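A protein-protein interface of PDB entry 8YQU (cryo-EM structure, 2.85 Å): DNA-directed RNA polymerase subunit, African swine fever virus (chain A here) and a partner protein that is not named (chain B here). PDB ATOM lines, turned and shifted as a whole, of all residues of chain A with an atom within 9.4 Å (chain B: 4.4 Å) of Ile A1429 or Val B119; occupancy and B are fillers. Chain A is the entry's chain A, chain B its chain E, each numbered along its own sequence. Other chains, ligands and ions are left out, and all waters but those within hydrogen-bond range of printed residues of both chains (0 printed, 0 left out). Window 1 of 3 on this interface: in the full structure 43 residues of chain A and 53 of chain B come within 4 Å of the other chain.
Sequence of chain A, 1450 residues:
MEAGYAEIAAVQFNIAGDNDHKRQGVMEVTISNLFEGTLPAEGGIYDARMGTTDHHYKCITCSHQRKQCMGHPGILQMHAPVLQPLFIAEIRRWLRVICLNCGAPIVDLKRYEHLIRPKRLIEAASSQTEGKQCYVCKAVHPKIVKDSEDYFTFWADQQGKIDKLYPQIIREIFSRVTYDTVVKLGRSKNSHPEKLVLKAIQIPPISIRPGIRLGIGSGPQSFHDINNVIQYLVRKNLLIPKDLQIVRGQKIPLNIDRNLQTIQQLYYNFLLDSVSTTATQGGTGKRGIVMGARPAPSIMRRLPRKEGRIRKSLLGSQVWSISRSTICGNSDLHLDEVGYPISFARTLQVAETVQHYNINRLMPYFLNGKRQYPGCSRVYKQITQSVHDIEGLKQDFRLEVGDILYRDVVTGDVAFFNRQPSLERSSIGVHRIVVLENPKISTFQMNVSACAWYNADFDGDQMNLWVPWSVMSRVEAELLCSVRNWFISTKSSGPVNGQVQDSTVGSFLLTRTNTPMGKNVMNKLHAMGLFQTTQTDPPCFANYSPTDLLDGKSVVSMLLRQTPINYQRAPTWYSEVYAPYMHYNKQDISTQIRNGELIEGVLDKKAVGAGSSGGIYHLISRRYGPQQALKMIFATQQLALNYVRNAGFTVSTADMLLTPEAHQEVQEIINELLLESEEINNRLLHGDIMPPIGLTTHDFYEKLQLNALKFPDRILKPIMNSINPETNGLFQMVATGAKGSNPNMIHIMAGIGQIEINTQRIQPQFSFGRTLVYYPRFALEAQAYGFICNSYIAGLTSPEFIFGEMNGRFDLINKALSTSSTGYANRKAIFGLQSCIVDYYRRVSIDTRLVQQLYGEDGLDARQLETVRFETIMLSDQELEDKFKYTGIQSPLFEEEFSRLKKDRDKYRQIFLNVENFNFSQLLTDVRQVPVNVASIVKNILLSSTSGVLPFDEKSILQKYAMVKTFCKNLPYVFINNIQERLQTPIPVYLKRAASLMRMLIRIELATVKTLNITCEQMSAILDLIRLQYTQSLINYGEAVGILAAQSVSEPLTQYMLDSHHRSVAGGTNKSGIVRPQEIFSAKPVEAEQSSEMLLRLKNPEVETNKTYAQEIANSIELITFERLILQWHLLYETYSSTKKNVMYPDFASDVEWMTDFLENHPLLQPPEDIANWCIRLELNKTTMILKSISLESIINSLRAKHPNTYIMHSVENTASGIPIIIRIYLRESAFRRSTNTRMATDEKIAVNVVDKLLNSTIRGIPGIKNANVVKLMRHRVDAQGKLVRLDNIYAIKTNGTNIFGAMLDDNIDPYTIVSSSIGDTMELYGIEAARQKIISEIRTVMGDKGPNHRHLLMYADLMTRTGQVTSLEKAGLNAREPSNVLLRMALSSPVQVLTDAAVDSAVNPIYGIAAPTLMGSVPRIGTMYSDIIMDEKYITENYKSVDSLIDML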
ATOM      1  N   MET A 472      10.236  -9.326 -25.448  1.00  0.00           N
ATOM      2  CA  MET A 472       8.955  -9.936 -25.791  1.00  0.00           C
ATOM      3  C   MET A 472       8.827 -10.156 -27.293  1.00  0.00           C
ATOM      4  O   MET A 472       8.373 -11.218 -27.735  1.00  0.00           O
ATOM      5  CB  MET A 472       7.806  -9.066 -25.284  1.00  0.00           C
ATOM      6  CG  MET A 472       7.626  -9.085 -23.780  1.00  0.00           C
ATOM      7  SD  MET A 472       5.909  -8.815 -23.310  1.00  0.00           S
ATOM      8  CE  MET A 472       5.869  -9.612 -21.711  1.00  0.00           C
ATOM      9  N   TYR A 840     -12.335 -20.675 -28.011  1.00  0.00           N
ATOM     10  CA  TYR A 840     -11.854 -21.817 -27.247  1.00  0.00           C
ATOM     11  C   TYR A 840     -12.580 -23.113 -27.578  1.00  0.00           C
ATOM     12  O   TYR A 840     -12.158 -24.176 -27.108  1.00  0.00           O
ATOM     13  CB  TYR A 840     -11.972 -21.529 -25.751  1.00  0.00           C
ATOM     14  CG  TYR A 840     -11.018 -20.460 -25.283  1.00  0.00           C
ATOM     15  CD1 TYR A 840      -9.648 -20.678 -25.281  1.00  0.00           C
ATOM     16  CD2 TYR A 840     -11.485 -19.226 -24.855  1.00  0.00           C
ATOM     17  CE1 TYR A 840      -8.774 -19.700 -24.862  1.00  0.00           C
ATOM     18  CE2 TYR A 840     -10.618 -18.245 -24.434  1.00  0.00           C
ATOM     19  CZ  TYR A 840      -9.263 -18.487 -24.438  1.00  0.00           C
ATOM     20  OH  TYR A 840      -8.396 -17.508 -24.016  1.00  0.00           O
ATOM     21  N   TYR A1037      -6.201 -21.672 -30.628  1.00  0.00           N
ATOM     22  CA  TYR A1037      -7.150 -20.713 -30.081  1.00  0.00           C
ATOM     23  C   TYR A1037      -6.726 -19.293 -30.435  1.00  0.00           C
ATOM     24  O   TYR A1037      -5.544 -18.948 -30.376  1.00  0.00           O
ATOM     25  CB  TYR A1037      -7.242 -20.856 -28.564  1.00  0.00           C
ATOM     26  CG  TYR A1037      -7.736 -22.200 -28.090  1.00  0.00           C
ATOM     27  CD1 TYR A1037      -8.694 -22.902 -28.803  1.00  0.00           C
ATOM     28  CD2 TYR A1037      -7.240 -22.768 -26.926  1.00  0.00           C
ATOM     29  CE1 TYR A1037      -9.147 -24.127 -28.367  1.00  0.00           C
ATOM     30  CE2 TYR A1037      -7.685 -23.994 -26.486  1.00  0.00           C
ATOM     31  CZ  TYR A1037      -8.638 -24.671 -27.210  1.00  0.00           C
ATOM     32  OH  TYR A1037      -9.087 -25.895 -26.775  1.00  0.00           O
ATOM     33  N   GLY A1423      -4.265 -14.281 -31.142  1.00  0.00           N
ATOM     34  CA  GLY A1423      -3.008 -14.997 -31.074  1.00  0.00           C
ATOM     35  C   GLY A1423      -2.407 -15.036 -29.686  1.00  0.00           C
ATOM     36  O   GLY A1423      -2.998 -15.603 -28.763  1.00  0.00           O
ATOM     37  N   THR A1424      -1.224 -14.437 -29.526  1.00  0.00           N
ATOM     38  CA  THR A1424      -0.571 -14.431 -28.222  1.00  0.00           C
ATOM     39  C   THR A1424      -1.362 -13.628 -27.199  1.00  0.00           C
ATOM     40  O   THR A1424      -1.249 -13.883 -25.995  1.00  0.00           O
ATOM     41  CB  THR A1424       0.847 -13.874 -28.340  1.00  0.00           C
ATOM     42  OG1 THR A1424       0.800 -12.549 -28.883  1.00  0.00           O
ATOM     43  CG2 THR A1424       1.689 -14.752 -29.241  1.00  0.00           C
ATOM     44  N   MET A1425      -2.161 -12.667 -27.651  1.00  0.00           N
ATOM     45  CA  MET A1425      -2.938 -11.822 -26.757  1.00  0.00           C
ATOM     46  C   MET A1425      -4.315 -12.398 -26.448  1.00  0.00           C
ATOM     47  O   MET A1425      -5.050 -11.806 -25.653  1.00  0.00           O
ATOM     48  CB  MET A1425      -3.102 -10.425 -27.362  1.00  0.00           C
ATOM     49  CG  MET A1425      -1.804  -9.650 -27.547  1.00  0.00           C
ATOM     50  SD  MET A1425      -0.883  -9.310 -26.038  1.00  0.00           S
ATOM     51  CE  MET A1425       0.416 -10.533 -26.155  1.00  0.00           C
ATOM     52  N   TYR A1426      -4.682 -13.528 -27.059  1.00  0.00           N
ATOM     53  CA  TYR A1426      -6.024 -14.070 -26.870  1.00  0.00           C
ATOM     54  C   TYR A1426      -6.236 -14.543 -25.438  1.00  0.00           C
ATOM     55  O   TYR A1426      -7.234 -14.190 -24.798  1.00  0.00           O
ATOM     56  CB  TYR A1426      -6.274 -15.212 -27.855  1.00  0.00           C
ATOM     57  CG  TYR A1426      -7.733 -15.576 -27.984  1.00  0.00           C
ATOM     58  CD1 TYR A1426      -8.619 -14.739 -28.644  1.00  0.00           C
ATOM     59  CD2 TYR A1426      -8.226 -16.754 -27.441  1.00  0.00           C
ATOM     60  CE1 TYR A1426      -9.953 -15.063 -28.762  1.00  0.00           C
ATOM     61  CE2 TYR A1426      -9.560 -17.087 -27.556  1.00  0.00           C
ATOM     62  CZ  TYR A1426     -10.418 -16.237 -28.217  1.00  0.00           C
ATOM     63  OH  TYR A1426     -11.748 -16.561 -28.334  1.00  0.00           O
ATOM     64  N   SER A1427      -5.313 -15.346 -24.920  1.00  0.00           N
ATOM     65  CA  SER A1427      -5.384 -15.837 -23.552  1.00  0.00           C
ATOM     66  C   SER A1427      -4.434 -15.027 -22.683  1.00  0.00           C
ATOM     67  O   SER A1427      -3.226 -15.002 -22.935  1.00  0.00           O
ATOM     68  CB  SER A1427      -5.026 -17.321 -23.483  1.00  0.00           C
ATOM     69  OG  SER A1427      -5.914 -18.099 -24.264  1.00  0.00           O
ATOM     70  N   ASP A1428      -4.979 -14.369 -21.667  1.00  0.00           N
ATOM     71  CA  ASP A1428      -4.157 -13.574 -20.771  1.00  0.00           C
ATOM     72  C   ASP A1428      -3.470 -14.467 -19.746  1.00  0.00           C
ATOM     73  O   ASP A1428      -3.885 -15.599 -19.489  1.00  0.00           O
ATOM     74  CB  ASP A1428      -4.989 -12.492 -20.078  1.00  0.00           C
ATOM     75  CG  ASP A1428      -6.207 -13.045 -19.367  1.00  0.00           C
ATOM     76  OD1 ASP A1428      -6.331 -14.280 -19.241  1.00  0.00           O
ATOM     77  OD2 ASP A1428      -7.049 -12.232 -18.932  1.00  0.00           O
ATOM     78  N   ILE A1429      -2.397 -13.942 -19.165  1.00  0.00           N
ATOM     79  CA  ILE A1429      -1.538 -14.692 -18.262  1.00  0.00           C
ATOM     80  C   ILE A1429      -1.658 -14.083 -16.875  1.00  0.00           C
ATOM     81  O   ILE A1429      -1.552 -12.861 -16.717  1.00  0.00           O
ATOM     82  CB  ILE A1429      -0.078 -14.683 -18.747  1.00  0.00           C
ATOM     83  CG1 ILE A1429       0.007 -15.256 -20.161  1.00  0.00           C
ATOM     84  CG2 ILE A1429       0.803 -15.473 -17.799  1.00  0.00           C
ATOM     85  CD1 ILE A1429      -0.473 -16.680 -20.277  1.00  0.00           C
ATOM     86  N   ILE A1430      -1.892 -14.926 -15.875  1.00  0.00           N
ATOM     87  CA  ILE A1430      -1.971 -14.480 -14.491  1.00  0.00           C
ATOM     88  C   ILE A1430      -0.793 -15.068 -13.730  1.00  0.00           C
ATOM     89  O   ILE A1430      -0.232 -16.100 -14.111  1.00  0.00           O
ATOM     90  CB  ILE A1430      -3.307 -14.868 -13.819  1.00  0.00           C
ATOM     91  CG1 ILE A1430      -3.365 -16.370 -13.554  1.00  0.00           C
ATOM     92  CG2 ILE A1430      -4.477 -14.450 -14.686  1.00  0.00           C
ATOM     93  CD1 ILE A1430      -4.521 -16.781 -12.675  1.00  0.00           C
ATOM     94  N   MET A1431      -0.413 -14.393 -12.652  1.00  0.00           N
ATOM     95  CA  MET A1431       0.739 -14.808 -11.869  1.00  0.00           C
ATOM     96  C   MET A1431       0.351 -15.942 -10.930  1.00  0.00           C
ATOM     97  O   MET A1431      -0.683 -15.886 -10.258  1.00  0.00           O
ATOM     98  CB  MET A1431       1.283 -13.628 -11.064  1.00  0.00           C
ATOM     99  CG  MET A1431       2.064 -12.615 -11.886  1.00  0.00           C
ATOM    100  SD  MET A1431       3.399 -13.294 -12.882  1.00  0.00           S
ATOM    101  CE  MET A1431       4.350 -14.170 -11.649  1.00  0.00           C
ATOM    102  N   ASP A1432       1.187 -16.976 -10.884  1.00  0.00           N
ATOM    103  CA  ASP A1432       0.918 -18.154 -10.060  1.00  0.00           C
ATOM    104  C   ASP A1432       1.221 -17.808  -8.607  1.00  0.00           C
ATOM    105  O   ASP A1432       2.358 -17.904  -8.143  1.00  0.00           O
ATOM    106  CB  ASP A1432       1.738 -19.345 -10.538  1.00  0.00           C
ATOM    107  CG  ASP A1432       1.119 -20.669 -10.149  1.00  0.00           C
ATOM    108  OD1 ASP A1432       0.159 -20.667  -9.350  1.00  0.00           O
ATOM    109  OD2 ASP A1432       1.585 -21.712 -10.649  1.00  0.00           O
ATOM    110  N   LEU B  71      -0.969 -26.680 -24.420  1.00  0.00           N
ATOM    111  CA  LEU B  71      -0.743 -25.281 -24.749  1.00  0.00           C
ATOM    112  C   LEU B  71      -0.690 -25.098 -26.259  1.00  0.00           C
ATOM    113  O   LEU B  71      -0.102 -25.907 -26.980  1.00  0.00           O
ATOM    114  CB  LEU B  71       0.559 -24.789 -24.120  1.00  0.00           C
ATOM    115  CG  LEU B  71       0.566 -24.512 -22.620  1.00  0.00           C
ATOM    116  CD1 LEU B  71       1.989 -24.516 -22.096  1.00  0.00           C
ATOM    117  CD2 LEU B  71      -0.102 -23.180 -22.339  1.00  0.00           C
ATOM    118  N   GLU B  75      -0.068 -19.525 -26.834  1.00  0.00           N
ATOM    119  CA  GLU B  75       0.016 -19.482 -25.377  1.00  0.00           C
ATOM    120  C   GLU B  75       1.426 -19.785 -24.889  1.00  0.00           C
ATOM    121  O   GLU B  75       1.915 -19.138 -23.958  1.00  0.00           O
ATOM    122  CB  GLU B  75      -0.987 -20.456 -24.762  1.00  0.00           C
ATOM    123  CG  GLU B  75      -2.430 -20.004 -24.873  1.00  0.00           C
ATOM    124  CD  GLU B  75      -3.415 -21.100 -24.519  1.00  0.00           C
ATOM    125  OE1 GLU B  75      -2.982 -22.258 -24.350  1.00  0.00           O
ATOM    126  OE2 GLU B  75      -4.622 -20.802 -24.411  1.00  0.00           O
ATOM    127  N   ARG B  78       3.535 -16.716 -25.577  1.00  0.00           N
ATOM    128  CA  ARG B  78       3.227 -15.659 -24.620  1.00  0.00           C
ATOM    129  C   ARG B  78       3.822 -15.962 -23.250  1.00  0.00           C
ATOM    130  O   ARG B  78       4.365 -15.068 -22.591  1.00  0.00           O
ATOM    131  CB  ARG B  78       1.715 -15.467 -24.525  1.00  0.00           C
ATOM    132  CG  ARG B  78       1.269 -14.491 -23.452  1.00  0.00           C
ATOM    133  CD  ARG B  78       1.641 -13.057 -23.781  1.00  0.00           C
ATOM    134  NE  ARG B  78       1.018 -12.126 -22.849  1.00  0.00           N
ATOM    135  CZ  ARG B  78       1.352 -10.849 -22.722  1.00  0.00           C
ATOM    136  NH1 ARG B  78       2.317 -10.312 -23.449  1.00  0.00           N
ATOM    137  NH2 ARG B  78       0.706 -10.095 -21.838  1.00  0.00           N
ATOM    138  N   LEU B  79       3.734 -17.218 -22.805  1.00  0.00           N
ATOM    139  CA  LEU B  79       4.326 -17.600 -21.527  1.00  0.00           C
ATOM    140  C   LEU B  79       5.830 -17.370 -21.528  1.00  0.00           C
ATOM    141  O   LEU B  79       6.384 -16.791 -20.585  1.00  0.00           O
ATOM    142  CB  LEU B  79       4.015 -19.064 -21.222  1.00  0.00           C
ATOM    143  CG  LEU B  79       2.595 -19.423 -20.792  1.00  0.00           C
ATOM    144  CD1 LEU B  79       2.441 -20.927 -20.712  1.00  0.00           C
ATOM    145  CD2 LEU B  79       2.293 -18.795 -19.451  1.00  0.00           C
ATOM    146  N   LEU B 117       3.680 -19.188 -13.794  1.00  0.00           N
ATOM    147  CA  LEU B 117       2.613 -18.517 -14.520  1.00  0.00           C
ATOM    148  C   LEU B 117       1.433 -19.465 -14.674  1.00  0.00           C
ATOM    149  O   LEU B 117       1.572 -20.685 -14.572  1.00  0.00           O
ATOM    150  CB  LEU B 117       3.075 -18.034 -15.903  1.00  0.00           C
ATOM    151  CG  LEU B 117       4.195 -16.995 -15.967  1.00  0.00           C
ATOM    152  CD1 LEU B 117       4.678 -16.823 -17.394  1.00  0.00           C
ATOM    153  CD2 LEU B 117       3.714 -15.672 -15.415  1.00  0.00           C
ATOM    154  N   LEU B 118       0.262 -18.882 -14.917  1.00  0.00           N
ATOM    155  CA  LEU B 118      -0.950 -19.634 -15.203  1.00  0.00           C
ATOM    156  C   LEU B 118      -1.645 -19.026 -16.411  1.00  0.00           C
ATOM    157  O   LEU B 118      -1.518 -17.829 -16.682  1.00  0.00           O
ATOM    158  CB  LEU B 118      -1.911 -19.648 -14.007  1.00  0.00           C
ATOM    159  CG  LEU B 118      -1.454 -20.361 -12.734  1.00  0.00           C
ATOM    160  CD1 LEU B 118      -2.532 -20.275 -11.670  1.00  0.00           C
ATOM    161  CD2 LEU B 118      -1.110 -21.809 -13.028  1.00  0.00           C
ATOM    162  N   VAL B 119      -2.377 -19.863 -17.139  1.00  0.00           N
ATOM    163  CA  VAL B 119      -3.113 -19.445 -18.326  1.00  0.00           C
ATOM    164  C   VAL B 119      -4.593 -19.430 -17.979  1.00  0.00           C
ATOM    165  O   VAL B 119      -5.174 -20.475 -17.658  1.00  0.00           O
ATOM    166  CB  VAL B 119      -2.837 -20.371 -19.521  1.00  0.00           C
ATOM    167  CG1 VAL B 119      -3.565 -19.869 -20.755  1.00  0.00           C
ATOM    168  CG2 VAL B 119      -1.344 -20.473 -19.779  1.00  0.00           C
ATOM    169  N   MET B 120      -5.205 -18.251 -18.045  1.00  0.00           N
ATOM    170  CA  MET B 120      -6.625 -18.090 -17.765  1.00  0.00           C
ATOM    171  C   MET B 120      -7.365 -17.914 -19.085  1.00  0.00           C
ATOM    172  O   MET B 120      -7.148 -16.929 -19.796  1.00  0.00           O
ATOM    173  CB  MET B 120      -6.873 -16.902 -16.838  1.00  0.00           C
ATOM    174  CG  MET B 120      -8.331 -16.720 -16.448  1.00  0.00           C
ATOM    175  SD  MET B 120      -8.641 -15.205 -15.524  1.00  0.00           S
ATOM    176  CE  MET B 120      -8.649 -13.999 -16.841  1.00  0.00           C
ATOM    177  N   ARG B 121      -8.233 -18.868 -19.405  1.00  0.00           N
ATOM    178  CA  ARG B 121      -8.964 -18.882 -20.668  1.00  0.00           C
ATOM    179  C   ARG B 121     -10.376 -18.368 -20.405  1.00  0.00           C
ATOM    180  O   ARG B 121     -11.220 -19.087 -19.866  1.00  0.00           O
ATOM    181  CB  ARG B 121      -8.969 -20.286 -21.264  1.00  0.00           C
ATOM    182  CG  ARG B 121      -7.598 -20.745 -21.735  1.00  0.00           C
ATOM    183  CD  ARG B 121      -7.595 -22.202 -22.160  1.00  0.00           C
ATOM    184  NE  ARG B 121      -6.330 -22.573 -22.783  1.00  0.00           N
ATOM    185  CZ  ARG B 121      -5.953 -23.818 -23.039  1.00  0.00           C
ATOM    186  NH1 ARG B 121      -6.716 -24.849 -22.722  1.00  0.00           N
ATOM    187  NH2 ARG B 121      -4.778 -24.033 -23.622  1.00  0.00           N
ATOM    188  N   GLU B 134     -11.386 -20.297 -17.340  1.00  0.00           N
ATOM    189  CA  GLU B 134     -10.729 -21.583 -17.134  1.00  0.00           C
ATOM    190  C   GLU B 134      -9.284 -21.328 -16.735  1.00  0.00           C
ATOM    191  O   GLU B 134      -8.561 -20.628 -17.449  1.00  0.00           O
ATOM    192  CB  GLU B 134     -10.785 -22.438 -18.401  1.00  0.00           C
ATOM    193  CG  GLU B 134     -12.158 -22.981 -18.733  1.00  0.00           C
ATOM    194  CD  GLU B 134     -12.096 -24.381 -19.297  1.00  0.00           C
ATOM    195  OE1 GLU B 134     -11.114 -25.092 -19.006  1.00  0.00           O
ATOM    196  OE2 GLU B 134     -13.026 -24.771 -20.033  1.00  0.00           O
ATOM    197  N   ILE B 135      -8.864 -21.898 -15.612  1.00  0.00           N
ATOM    198  CA  ILE B 135      -7.501 -21.741 -15.112  1.00  0.00           C
ATOM    199  C   ILE B 135      -6.730 -23.010 -15.448  1.00  0.00           C
ATOM    200  O   ILE B 135      -7.084 -24.103 -14.993  1.00  0.00           O
ATOM    201  CB  ILE B 135      -7.475 -21.456 -13.607  1.00  0.00           C
ATOM    202  CG1 ILE B 135      -8.288 -20.202 -13.287  1.00  0.00           C
ATOM    203  CG2 ILE B 135      -6.042 -21.299 -13.126  1.00  0.00           C
ATOM    204  CD1 ILE B 135      -7.612 -18.922 -13.711  1.00  0.00           C
ATOM    205  N   TRP B 136      -5.673 -22.868 -16.241  1.00  0.00           N
ATOM    206  CA  TRP B 136      -4.852 -23.988 -16.671  1.00  0.00           C
ATOM    207  C   TRP B 136      -3.417 -23.794 -16.203  1.00  0.00           C
ATOM    208  O   TRP B 136      -2.877 -22.684 -16.262  1.00  0.00           O
ATOM    209  CB  TRP B 136      -4.894 -24.146 -18.193  1.00  0.00           C
ATOM    210  CG  TRP B 136      -6.109 -24.870 -18.680  1.00  0.00           C
ATOM    211  CD1 TRP B 136      -7.263 -24.313 -19.145  1.00  0.00           C
ATOM    212  CD2 TRP B 136      -6.290 -26.288 -18.749  1.00  0.00           C
ATOM    213  NE1 TRP B 136      -8.152 -25.298 -19.500  1.00  0.00           N
ATOM    214  CE2 TRP B 136      -7.579 -26.519 -19.266  1.00  0.00           C
ATOM    215  CE3 TRP B 136      -5.488 -27.386 -18.423  1.00  0.00           C
ATOM    216  CZ2 TRP B 136      -8.083 -27.801 -19.467  1.00  0.00           C
ATOM    217  CZ3 TRP B 136      -5.990 -28.656 -18.623  1.00  0.00           C
ATOM    218  CH2 TRP B 136      -7.275 -28.854 -19.139  1.00  0.00           C
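N of Met B120 sits at hydrogen-bond distance from O of Asp A1428, at 3.3 Å.
OG of Ser A1427 sits at hydrogen-bond distance from OE2 of Glu B75 (3.0 Å).
N of Leu B118 sits at hydrogen-bond distance from O of Ile A1430, 2.9 Å away.
The backbone NH (N) of Arg B121 lies within hydrogen-bond range of the backbone carbonyl oxygen (O) of Glu B134, at 2.7 Å.
The side-chain hydroxyl (OH) of Tyr A840 sits at hydrogen-bond distance from the side-chain hydroxyl (OG) of Ser A1427, at 2.6 Å.
The backbone NH of Trp B136 lies within hydrogen-bond range of the backbone carbonyl oxygen of Val B119.
The side-chain carboxylate (OE1) of Glu B75 lies within salt-bridge range of the guanidinium group (NH2) of Arg B121.
Among the printed residues, merely in contact across the chains: Met A1425 with Arg B78 (3.3 Å), Met A1431 with Leu B117 (3.5 Å), Ile A1429 with Leu B118 (3.5 Å), Tyr A840 with Arg B121 (3.5 Å), Asp A1432 with Leu B118 (3.6 Å), Ile A1429 with Leu B79 (3.6 Å), Ile A1429 with Arg B78 (3.6 Å), Thr A1424 with Arg B78 (3.6 Å), Ile A1430 with Leu B117 (3.8 Å), Ile A1429 with Leu B117 (3.8 Å), Asp A1432 with Leu B117 (3.8 Å), Tyr A1037 with Arg B121 (3.9 Å), Met A472 with Arg B78 (3.9 Å), Ile A1430 with Ile B135 (3.9 Å) and Ile A1429 with Val B119 (3.9 Å).
Ile A1429 touches just these residues of chain B: Arg B78, Leu B79, Leu B117, Leu B118 and Val B119.
Printed residues of chain A within 4 Å of Val B119: Ile A1429.
Printed residues of chain B within 4 Å of Tyr A1037: Arg B121 (3.9 Å).
Printed residues of chain A within 4 Å of Met B120: Asp A1428 (2.8 Å).
Of the printed residues of chain B, Ser A1427 touches Glu B75.
Printed residues of chain B within 4 Å of Asp A1432: Leu B117 and Leu B118.
Printed residues of chain B within 4 Å of Asp A1428: Met B120.
Glu B134 touches none of the printed residues of chain A.
Trp B136 touches none of the printed residues of chain A.
The nearest printed residue of chain B that does not touch Ile A1429 is Glu B75 (5.0 Å).
The nearest printed residue of chain A that does not touch Val B119 is Ser A1427 (4.01 Å).
The nearest printed residue of chain B that does not touch Ser A1427 is Val B119 (4.01 Å).
Of the 12 printed residues of chain B, 9 touch a printed residue of chain A.
Hydrophobic or aromatic side chains of chain B within 4 Å of the printed part of chain A: Leu B79, Leu B117, Leu B118, Val B119, Met B120 and Ile B135.
Hydrophobic or aromatic side chains of chain A within 4 Å of the printed part of chain B: Met A472, Tyr A840, Tyr A1037, Met A1425, Ile A1429, Ile A1430 and Met A1431.
Among the printed residues, no Asp or Glu carboxylate lies within 4 Å of a Lys or Arg side-chain nitrogen of the other chain.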
